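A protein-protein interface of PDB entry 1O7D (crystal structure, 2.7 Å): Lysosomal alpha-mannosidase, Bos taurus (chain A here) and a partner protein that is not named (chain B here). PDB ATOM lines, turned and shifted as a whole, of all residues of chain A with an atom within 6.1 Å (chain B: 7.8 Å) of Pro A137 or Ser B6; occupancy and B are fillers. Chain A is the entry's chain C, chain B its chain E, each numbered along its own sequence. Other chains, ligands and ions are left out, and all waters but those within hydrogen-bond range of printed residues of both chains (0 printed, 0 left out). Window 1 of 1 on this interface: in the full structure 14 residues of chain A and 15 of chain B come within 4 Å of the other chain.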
ATOM      1  N   ASN A  86     -15.761 -21.887  -5.194  1.00  0.00           N
ATOM      2  CA  ASN A  86     -15.222 -23.232  -5.351  1.00  0.00           C
ATOM      3  C   ASN A  86     -16.315 -24.272  -5.157  1.00  0.00           C
ATOM      4  O   ASN A  86     -16.905 -24.370  -4.085  1.00  0.00           O
ATOM      5  CB  ASN A  86     -14.097 -23.450  -4.344  1.00  0.00           C
ATOM      6  CG  ASN A  86     -13.698 -24.893  -4.221  1.00  0.00           C
ATOM      7  OD1 ASN A  86     -13.631 -25.618  -5.196  1.00  0.00           O
ATOM      8  ND2 ASN A  86     -13.411 -25.312  -3.011  1.00  0.00           N
ATOM      9  N   PRO A  87     -16.610 -25.054  -6.202  1.00  0.00           N
ATOM     10  CA  PRO A  87     -17.630 -26.105  -6.194  1.00  0.00           C
ATOM     11  C   PRO A  87     -17.205 -27.446  -5.586  1.00  0.00           C
ATOM     12  O   PRO A  87     -18.051 -28.305  -5.368  1.00  0.00           O
ATOM     13  CB  PRO A  87     -17.971 -26.268  -7.672  1.00  0.00           C
ATOM     14  CG  PRO A  87     -17.521 -25.009  -8.281  1.00  0.00           C
ATOM     15  CD  PRO A  87     -16.242 -24.733  -7.582  1.00  0.00           C
ATOM     16  N   LEU A  88     -15.913 -27.633  -5.325  1.00  0.00           N
ATOM     17  CA  LEU A  88     -15.415 -28.889  -4.780  1.00  0.00           C
ATOM     18  C   LEU A  88     -15.643 -29.072  -3.295  1.00  0.00           C
ATOM     19  O   LEU A  88     -15.681 -28.108  -2.546  1.00  0.00           O
ATOM     20  CB  LEU A  88     -13.932 -29.047  -5.095  1.00  0.00           C
ATOM     21  CG  LEU A  88     -13.601 -29.468  -6.531  1.00  0.00           C
ATOM     22  CD1 LEU A  88     -12.100 -29.481  -6.735  1.00  0.00           C
ATOM     23  CD2 LEU A  88     -14.167 -30.856  -6.798  1.00  0.00           C
ATOM     24  N   ARG A  90     -13.832 -29.769  -1.037  1.00  0.00           N
ATOM     25  CA  ARG A  90     -12.612 -29.533  -0.273  1.00  0.00           C
ATOM     26  C   ARG A  90     -12.094 -28.153  -0.641  1.00  0.00           C
ATOM     27  O   ARG A  90     -12.562 -27.539  -1.596  1.00  0.00           O
ATOM     28  CB  ARG A  90     -11.578 -30.610  -0.573  1.00  0.00           C
ATOM     29  CG  ARG A  90     -12.014 -31.966  -0.039  1.00  0.00           C
ATOM     30  CD  ARG A  90     -11.133 -33.109  -0.518  1.00  0.00           C
ATOM     31  NE  ARG A  90     -11.409 -33.434  -1.912  1.00  0.00           N
ATOM     32  CZ  ARG A  90     -12.576 -33.894  -2.348  1.00  0.00           C
ATOM     33  NH1 ARG A  90     -13.563 -34.088  -1.488  1.00  0.00           N
ATOM     34  NH2 ARG A  90     -12.766 -34.135  -3.642  1.00  0.00           N
ATOM     35  N   LYS A  91     -11.134 -27.657   0.125  1.00  0.00           N
ATOM     36  CA  LYS A  91     -10.591 -26.324  -0.099  1.00  0.00           C
ATOM     37  C   LYS A  91      -9.715 -26.278  -1.345  1.00  0.00           C
ATOM     38  O   LYS A  91      -9.103 -27.281  -1.728  1.00  0.00           O
ATOM     39  CB  LYS A  91      -9.777 -25.898   1.130  1.00  0.00           C
ATOM     40  CG  LYS A  91      -8.589 -26.830   1.390  1.00  0.00           C
ATOM     41  CD  LYS A  91      -7.982 -26.672   2.786  1.00  0.00           C
ATOM     42  CE  LYS A  91      -6.856 -27.715   3.004  1.00  0.00           C
ATOM     43  NZ  LYS A  91      -6.144 -27.669   4.336  1.00  0.00           N
ATOM     44  N   VAL A  92      -9.668 -25.109  -1.978  1.00  0.00           N
ATOM     45  CA  VAL A  92      -8.831 -24.916  -3.160  1.00  0.00           C
ATOM     46  C   VAL A  92      -7.850 -23.780  -2.900  1.00  0.00           C
ATOM     47  O   VAL A  92      -8.157 -22.828  -2.178  1.00  0.00           O
ATOM     48  CB  VAL A  92      -9.669 -24.576  -4.432  1.00  0.00           C
ATOM     49  CG1 VAL A  92      -8.759 -24.067  -5.534  1.00  0.00           C
ATOM     50  CG2 VAL A  92     -10.393 -25.824  -4.926  1.00  0.00           C
ATOM     51  N   LEU A 135      -7.229 -18.745  -1.756  1.00  0.00           N
ATOM     52  CA  LEU A 135      -7.602 -19.891  -0.929  1.00  0.00           C
ATOM     53  C   LEU A 135      -9.132 -19.887  -0.735  1.00  0.00           C
ATOM     54  O   LEU A 135      -9.696 -18.961  -0.147  1.00  0.00           O
ATOM     55  CB  LEU A 135      -6.884 -19.813   0.414  1.00  0.00           C
ATOM     56  CG  LEU A 135      -5.409 -19.428   0.308  1.00  0.00           C
ATOM     57  CD1 LEU A 135      -4.747 -19.569   1.666  1.00  0.00           C
ATOM     58  CD2 LEU A 135      -4.720 -20.308  -0.709  1.00  0.00           C
ATOM     59  N   VAL A 136      -9.795 -20.916  -1.252  1.00  0.00           N
ATOM     60  CA  VAL A 136     -11.244 -21.012  -1.161  1.00  0.00           C
ATOM     61  C   VAL A 136     -11.749 -22.274  -0.463  1.00  0.00           C
ATOM     62  O   VAL A 136     -11.294 -23.391  -0.747  1.00  0.00           O
ATOM     63  CB  VAL A 136     -11.872 -20.947  -2.554  1.00  0.00           C
ATOM     64  CG1 VAL A 136     -13.384 -20.887  -2.444  1.00  0.00           C
ATOM     65  CG2 VAL A 136     -11.347 -19.736  -3.291  1.00  0.00           C
ATOM     66  N   PRO A 137     -12.712 -22.110   0.459  1.00  0.00           N
ATOM     67  CA  PRO A 137     -13.306 -23.213   1.219  1.00  0.00           C
ATOM     68  C   PRO A 137     -14.163 -24.098   0.324  1.00  0.00           C
ATOM     69  O   PRO A 137     -14.636 -23.659  -0.727  1.00  0.00           O
ATOM     70  CB  PRO A 137     -14.158 -22.498   2.262  1.00  0.00           C
ATOM     71  CG  PRO A 137     -13.534 -21.151   2.369  1.00  0.00           C
ATOM     72  CD  PRO A 137     -13.232 -20.823   0.941  1.00  0.00           C
ATOM     73  N   ALA A 138     -14.368 -25.338   0.744  1.00  0.00           N
ATOM     74  CA  ALA A 138     -15.190 -26.255  -0.026  1.00  0.00           C
ATOM     75  C   ALA A 138     -16.623 -25.712  -0.090  1.00  0.00           C
ATOM     76  O   ALA A 138     -17.135 -25.176   0.893  1.00  0.00           O
ATOM     77  CB  ALA A 138     -15.168 -27.627   0.619  1.00  0.00           C
ATOM     78  N   VAL A 139     -17.248 -25.829  -1.257  1.00  0.00           N
ATOM     79  CA  VAL A 139     -18.617 -25.360  -1.456  1.00  0.00           C
ATOM     80  C   VAL A 139     -18.777 -23.912  -1.014  1.00  0.00           C
ATOM     81  O   VAL A 139     -19.866 -23.494  -0.644  1.00  0.00           O
ATOM     82  CB  VAL A 139     -19.613 -26.221  -0.666  1.00  0.00           C
ATOM     83  CG1 VAL A 139     -21.024 -25.768  -0.928  1.00  0.00           C
ATOM     84  CG2 VAL A 139     -19.474 -27.665  -1.065  1.00  0.00           C
ATOM     85  N   GLY A 140     -17.686 -23.148  -1.049  1.00  0.00           N
ATOM     86  CA  GLY A 140     -17.749 -21.752  -0.647  1.00  0.00           C
ATOM     87  C   GLY A 140     -17.108 -20.752  -1.600  1.00  0.00           C
ATOM     88  O   GLY A 140     -17.009 -20.968  -2.809  1.00  0.00           O
ATOM     89  N   PHE A 141     -16.673 -19.632  -1.034  1.00  0.00           N
ATOM     90  CA  PHE A 141     -16.043 -18.577  -1.800  1.00  0.00           C
ATOM     91  C   PHE A 141     -15.204 -17.664  -0.918  1.00  0.00           C
ATOM     92  O   PHE A 141     -15.308 -17.679   0.319  1.00  0.00           O
ATOM     93  CB  PHE A 141     -17.109 -17.745  -2.509  1.00  0.00           C
ATOM     94  CG  PHE A 141     -18.104 -17.090  -1.580  1.00  0.00           C
ATOM     95  CD1 PHE A 141     -17.699 -16.145  -0.646  1.00  0.00           C
ATOM     96  CD2 PHE A 141     -19.453 -17.402  -1.662  1.00  0.00           C
ATOM     97  CE1 PHE A 141     -18.623 -15.520   0.183  1.00  0.00           C
ATOM     98  CE2 PHE A 141     -20.381 -16.781  -0.839  1.00  0.00           C
ATOM     99  CZ  PHE A 141     -19.965 -15.840   0.086  1.00  0.00           C
ATOM    100  N   SER A 142     -14.383 -16.853  -1.574  1.00  0.00           N
ATOM    101  CA  SER A 142     -13.518 -15.893  -0.897  1.00  0.00           C
ATOM    102  C   SER A 142     -13.548 -14.591  -1.681  1.00  0.00           C
ATOM    103  O   SER A 142     -13.661 -14.595  -2.907  1.00  0.00           O
ATOM    104  CB  SER A 142     -12.077 -16.399  -0.841  1.00  0.00           C
ATOM    105  OG  SER A 142     -11.951 -17.480   0.052  1.00  0.00           O
ATOM    106  N   ARG B   2     -19.033 -10.019   4.620  1.00  0.00           N
ATOM    107  CA  ARG B   2     -18.897 -11.486   4.690  1.00  0.00           C
ATOM    108  C   ARG B   2     -17.878 -11.873   3.620  1.00  0.00           C
ATOM    109  O   ARG B   2     -18.219 -12.235   2.489  1.00  0.00           O
ATOM    110  CB  ARG B   2     -20.222 -12.199   4.455  1.00  0.00           C
ATOM    111  CG  ARG B   2     -20.108 -13.729   4.502  1.00  0.00           C
ATOM    112  CD  ARG B   2     -19.604 -14.234   5.845  1.00  0.00           C
ATOM    113  NE  ARG B   2     -20.002 -15.618   6.092  1.00  0.00           N
ATOM    114  CZ  ARG B   2     -21.231 -16.087   5.886  1.00  0.00           C
ATOM    115  NH1 ARG B   2     -22.196 -15.294   5.412  1.00  0.00           N
ATOM    116  NH2 ARG B   2     -21.507 -17.348   6.189  1.00  0.00           N
ATOM    117  N   THR B   3     -16.612 -11.788   3.995  1.00  0.00           N
ATOM    118  CA  THR B   3     -15.565 -12.065   3.052  1.00  0.00           C
ATOM    119  C   THR B   3     -15.463 -13.488   2.579  1.00  0.00           C
ATOM    120  O   THR B   3     -15.118 -13.745   1.427  1.00  0.00           O
ATOM    121  CB  THR B   3     -14.207 -11.771   3.604  1.00  0.00           C
ATOM    122  OG1 THR B   3     -14.159 -10.476   4.227  1.00  0.00           O
ATOM    123  CG2 THR B   3     -13.273 -11.810   2.471  1.00  0.00           C
ATOM    124  N   GLN B   4     -15.769 -14.419   3.458  1.00  0.00           N
ATOM    125  CA  GLN B   4     -15.603 -15.802   3.108  1.00  0.00           C
ATOM    126  C   GLN B   4     -16.731 -16.706   3.601  1.00  0.00           C
ATOM    127  O   GLN B   4     -17.169 -16.596   4.747  1.00  0.00           O
ATOM    128  CB  GLN B   4     -14.266 -16.205   3.686  1.00  0.00           C
ATOM    129  CG  GLN B   4     -13.821 -17.592   3.432  1.00  0.00           C
ATOM    130  CD  GLN B   4     -12.338 -17.717   3.735  1.00  0.00           C
ATOM    131  OE1 GLN B   4     -11.482 -17.537   2.864  1.00  0.00           O
ATOM    132  NE2 GLN B   4     -12.027 -17.995   4.986  1.00  0.00           N
ATOM    133  N   PHE B   5     -17.188 -17.599   2.724  1.00  0.00           N
ATOM    134  CA  PHE B   5     -18.273 -18.538   3.025  1.00  0.00           C
ATOM    135  C   PHE B   5     -17.797 -19.981   2.777  1.00  0.00           C
ATOM    136  O   PHE B   5     -16.675 -20.210   2.305  1.00  0.00           O
ATOM    137  CB  PHE B   5     -19.485 -18.228   2.122  1.00  0.00           C
ATOM    138  CG  PHE B   5     -20.653 -19.175   2.300  1.00  0.00           C
ATOM    139  CD1 PHE B   5     -21.500 -19.066   3.406  1.00  0.00           C
ATOM    140  CD2 PHE B   5     -20.882 -20.203   1.379  1.00  0.00           C
ATOM    141  CE1 PHE B   5     -22.551 -19.960   3.600  1.00  0.00           C
ATOM    142  CE2 PHE B   5     -21.946 -21.117   1.569  1.00  0.00           C
ATOM    143  CZ  PHE B   5     -22.778 -20.988   2.684  1.00  0.00           C
ATOM    144  N   SER B   6     -18.660 -20.937   3.112  1.00  0.00           N
ATOM    145  CA  SER B   6     -18.433 -22.365   2.939  1.00  0.00           C
ATOM    146  C   SER B   6     -19.821 -22.943   3.148  1.00  0.00           C
ATOM    147  O   SER B   6     -20.610 -22.365   3.900  1.00  0.00           O
ATOM    148  CB  SER B   6     -17.498 -22.884   4.003  1.00  0.00           C
ATOM    149  OG  SER B   6     -17.456 -24.295   3.982  1.00  0.00           O
ATOM    150  N   GLY B   7     -20.146 -24.065   2.524  1.00  0.00           N
ATOM    151  CA  GLY B   7     -21.478 -24.608   2.728  1.00  0.00           C
ATOM    152  C   GLY B   7     -21.461 -25.810   3.641  1.00  0.00           C
ATOM    153  O   GLY B   7     -22.503 -26.298   4.072  1.00  0.00           O
ATOM    154  N   LEU B   8     -20.256 -26.268   3.944  1.00  0.00           N
ATOM    155  CA  LEU B   8     -20.069 -27.443   4.771  1.00  0.00           C
ATOM    156  C   LEU B   8     -19.482 -27.120   6.140  1.00  0.00           C
ATOM    157  O   LEU B   8     -18.781 -26.135   6.315  1.00  0.00           O
ATOM    158  CB  LEU B   8     -19.151 -28.422   4.035  1.00  0.00           C
ATOM    159  CG  LEU B   8     -19.398 -28.583   2.537  1.00  0.00           C
ATOM    160  CD1 LEU B   8     -18.405 -29.600   1.958  1.00  0.00           C
ATOM    161  CD2 LEU B   8     -20.843 -29.045   2.312  1.00  0.00           C
ATOM    162  N   ARG B   9     -19.782 -27.966   7.115  1.00  0.00           N
ATOM    163  CA  ARG B   9     -19.259 -27.787   8.459  1.00  0.00           C
ATOM    164  C   ARG B   9     -17.987 -28.609   8.548  1.00  0.00           C
ATOM    165  O   ARG B   9     -17.056 -28.244   9.257  1.00  0.00           O
ATOM    166  CB  ARG B   9     -20.266 -28.276   9.494  1.00  0.00           C
ATOM    167  N   ARG B  10     -17.961 -29.727   7.825  1.00  0.00           N
ATOM    168  CA  ARG B  10     -16.797 -30.619   7.787  1.00  0.00           C
ATOM    169  C   ARG B  10     -16.670 -31.059   6.325  1.00  0.00           C
ATOM    170  O   ARG B  10     -17.614 -31.602   5.757  1.00  0.00           O
ATOM    171  CB  ARG B  10     -17.018 -31.837   8.721  1.00  0.00           C
ATOM    172  N   GLU B  11     -15.523 -30.809   5.703  1.00  0.00           N
ATOM    173  CA  GLU B  11     -15.362 -31.173   4.299  1.00  0.00           C
ATOM    174  C   GLU B  11     -15.329 -32.656   3.964  1.00  0.00           C
ATOM    175  O   GLU B  11     -15.006 -33.495   4.798  1.00  0.00           O
ATOM    176  CB  GLU B  11     -14.126 -30.488   3.692  1.00  0.00           C
ATOM    177  CG  GLU B  11     -12.829 -30.570   4.468  1.00  0.00           C
ATOM    178  CD  GLU B  11     -11.685 -29.841   3.745  1.00  0.00           C
ATOM    179  OE1 GLU B  11     -11.866 -28.665   3.304  1.00  0.00           O
ATOM    180  OE2 GLU B  11     -10.596 -30.451   3.629  1.00  0.00           O
ATOM    181  N   LEU B  58     -23.617 -31.935   7.820  1.00  0.00           N
ATOM    182  CA  LEU B  58     -22.525 -31.878   6.830  1.00  0.00           C
ATOM    183  C   LEU B  58     -22.601 -30.454   6.255  1.00  0.00           C
ATOM    184  O   LEU B  58     -21.583 -29.785   6.056  1.00  0.00           O
ATOM    185  CB  LEU B  58     -22.729 -32.897   5.696  1.00  0.00           C
ATOM    186  CG  LEU B  58     -21.658 -32.826   4.587  1.00  0.00           C
ATOM    187  CD1 LEU B  58     -20.344 -33.372   5.127  1.00  0.00           C
ATOM    188  CD2 LEU B  58     -22.092 -33.613   3.369  1.00  0.00           C
ATOM    189  N   PHE B  59     -23.840 -30.006   6.050  1.00  0.00           N
ATOM    190  CA  PHE B  59     -24.141 -28.691   5.509  1.00  0.00           C
ATOM    191  C   PHE B  59     -24.548 -27.698   6.600  1.00  0.00           C
ATOM    192  O   PHE B  59     -25.288 -28.036   7.519  1.00  0.00           O
ATOM    193  CB  PHE B  59     -25.285 -28.801   4.497  1.00  0.00           C
ATOM    194  CG  PHE B  59     -24.937 -29.571   3.262  1.00  0.00           C
ATOM    195  CD1 PHE B  59     -24.268 -28.959   2.206  1.00  0.00           C
ATOM    196  CD2 PHE B  59     -25.272 -30.909   3.150  1.00  0.00           C
ATOM    197  CE1 PHE B  59     -23.937 -29.674   1.053  1.00  0.00           C
ATOM    198  CE2 PHE B  59     -24.944 -31.630   2.003  1.00  0.00           C
ATOM    199  CZ  PHE B  59     -24.278 -31.014   0.955  1.00  0.00           C
ATOM    200  N   SER B  60     -24.085 -26.463   6.451  1.00  0.00           N
ATOM    201  CA  SER B  60     -24.367 -25.378   7.376  1.00  0.00           C
ATOM    202  C   SER B  60     -25.408 -24.406   6.796  1.00  0.00           C
ATOM    203  O   SER B  60     -26.302 -23.941   7.508  1.00  0.00           O
ATOM    204  CB  SER B  60     -23.070 -24.609   7.667  1.00  0.00           C
ATOM    205  OG  SER B  60     -22.564 -23.967   6.495  1.00  0.00           O
ATOM    206  N   ALA B  61     -25.282 -24.090   5.508  1.00  0.00           N
ATOM    207  CA  ALA B  61     -26.192 -23.151   4.843  1.00  0.00           C
ATOM    208  C   ALA B  61     -27.661 -23.438   5.094  1.00  0.00           C
ATOM    209  O   ALA B  61     -28.483 -22.512   5.151  1.00  0.00           O
ATOM    210  CB  ALA B  61     -25.932 -23.143   3.350  1.00  0.00           C
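O of Val A139 is in hydrogen-bond range of N of Gly B7, 3.2 Å away.
OE1 of Gln B4 sits at hydrogen-bond distance from OG of Ser A142 (2.9 Å).
The backbone carbonyl oxygen of Ala A138 is in hydrogen-bond range of the side-chain hydroxyl of Ser B6, at 3.2 Å.
The backbone carbonyl oxygen (O) of Phe A141 lies within hydrogen-bond range of the backbone NH (N) of Phe B5, at 3.1 Å.
The backbone NH (N) of Lys A91 is in hydrogen-bond range of the side-chain carboxylate (OE1) of Glu B11, 3.4 Å away.
Printed residues of chain B that touch a printed residue of chain A: Thr B3, Gln B4, Phe B5, Ser B6, Gly B7, Leu B8 and Glu B11.
Hydrophobic or aromatic side chains of chain B within 4 Å of the printed part of chain A: Phe B5 and Leu B8.
Of the 14 printed residues of chain A, 9 touch a printed residue of chain B.
Printed residues of chain A that touch a printed residue of chain B: Arg A90, Lys A91, Leu A135, Pro A137, Ala A138, Val A139, Gly A140, Phe A141 and Ser A142.
Hydrophobic or aromatic side chains of chain A that line the printed part of chain B: Pro A137, Val A139 and Phe A141.
Among the printed residues, 18 pairs touch across the chains.
Pro A137 touches just these residues of chain B: Gln B4 (3.7 Å), Phe B5 (3.3 Å) and Ser B6 (3.8 Å).
Ser B6 touches four residues of chain A.
Ala A138 touches just these residues of chain B: Ser B6 (3.2 Å) and Gly B7 (3.6 Å).
Of the printed residues of chain A, Phe B5 touches Pro A137, Val A139, Gly A140 and Phe A141.
Of the printed residues of chain B, Ser A142 touches Thr B3 and Gln B4.
Printed residues of chain A within 4 Å of Glu B11: Arg A90 and Lys A91.
Of the printed residues of chain A, Gln B4 touches Leu A135, Pro A137, Phe A141 and Ser A142.
Ala B61 touches none of the printed residues of chain A.
Arg B9 touches none of the printed residues of chain A.
The nearest residue of chain B that does not touch Pro A137 is Glu B11 (5.9 Å).
The nearest residue of chain A that does not touch Ser B6 is Phe A141 (4.8 Å).
The nearest printed residue of chain B that does not touch Val A139 is Phe B59 (5.3 Å).
Gln B4 touches Leu A135.
CG of Pro A137 touches CG of Gln B4, 3.7 Å away.
Ser B6 touches Pro A137.
Gly B7 touches Ala A138 (N to O, 3.6 Å).
O of Val A139 touches CE2 of Phe B5, at 3.9 Å.
Val A139 touches Leu B8 (CG2 to CG, 3.7 Å).
Phe B5 touches Gly A140.
Gly A140 touches Ser B6 (CA to CA, 3.7 Å).
Phe A141 touches Gln B4 (O to CA, 3.4 Å).
CA of Ser A142 touches O of Thr B3, at 3.5 Å.
The side-chain hydroxyl of Ser B6 lies within hydrogen-bond range of the backbone carbonyl oxygen of Leu B8 (3.3 Å).
The backbone carbonyl oxygen (O) of Gln B4 sits at hydrogen-bond distance from the guanidinium group (NE) of Arg B2 (3.3 Å).
The backbone carbonyl oxygen of Leu A88 is in hydrogen-bond range of the backbone NH of Val A139 (3.1 Å).
The backbone carbonyl oxygen (O) of Gly B7 lies within hydrogen-bond range of the backbone NH (N) of Ser B60 (2.9 Å).
The side-chain amide nitrogen (ND2) of Asn A86 sits at hydrogen-bond distance from the backbone carbonyl oxygen (O) of Arg A90, 2.8 Å away.
The side-chain hydroxyl (OG) of Ser A142 is in hydrogen-bond range of the backbone carbonyl oxygen (O) of Leu A135 (2.7 Å).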
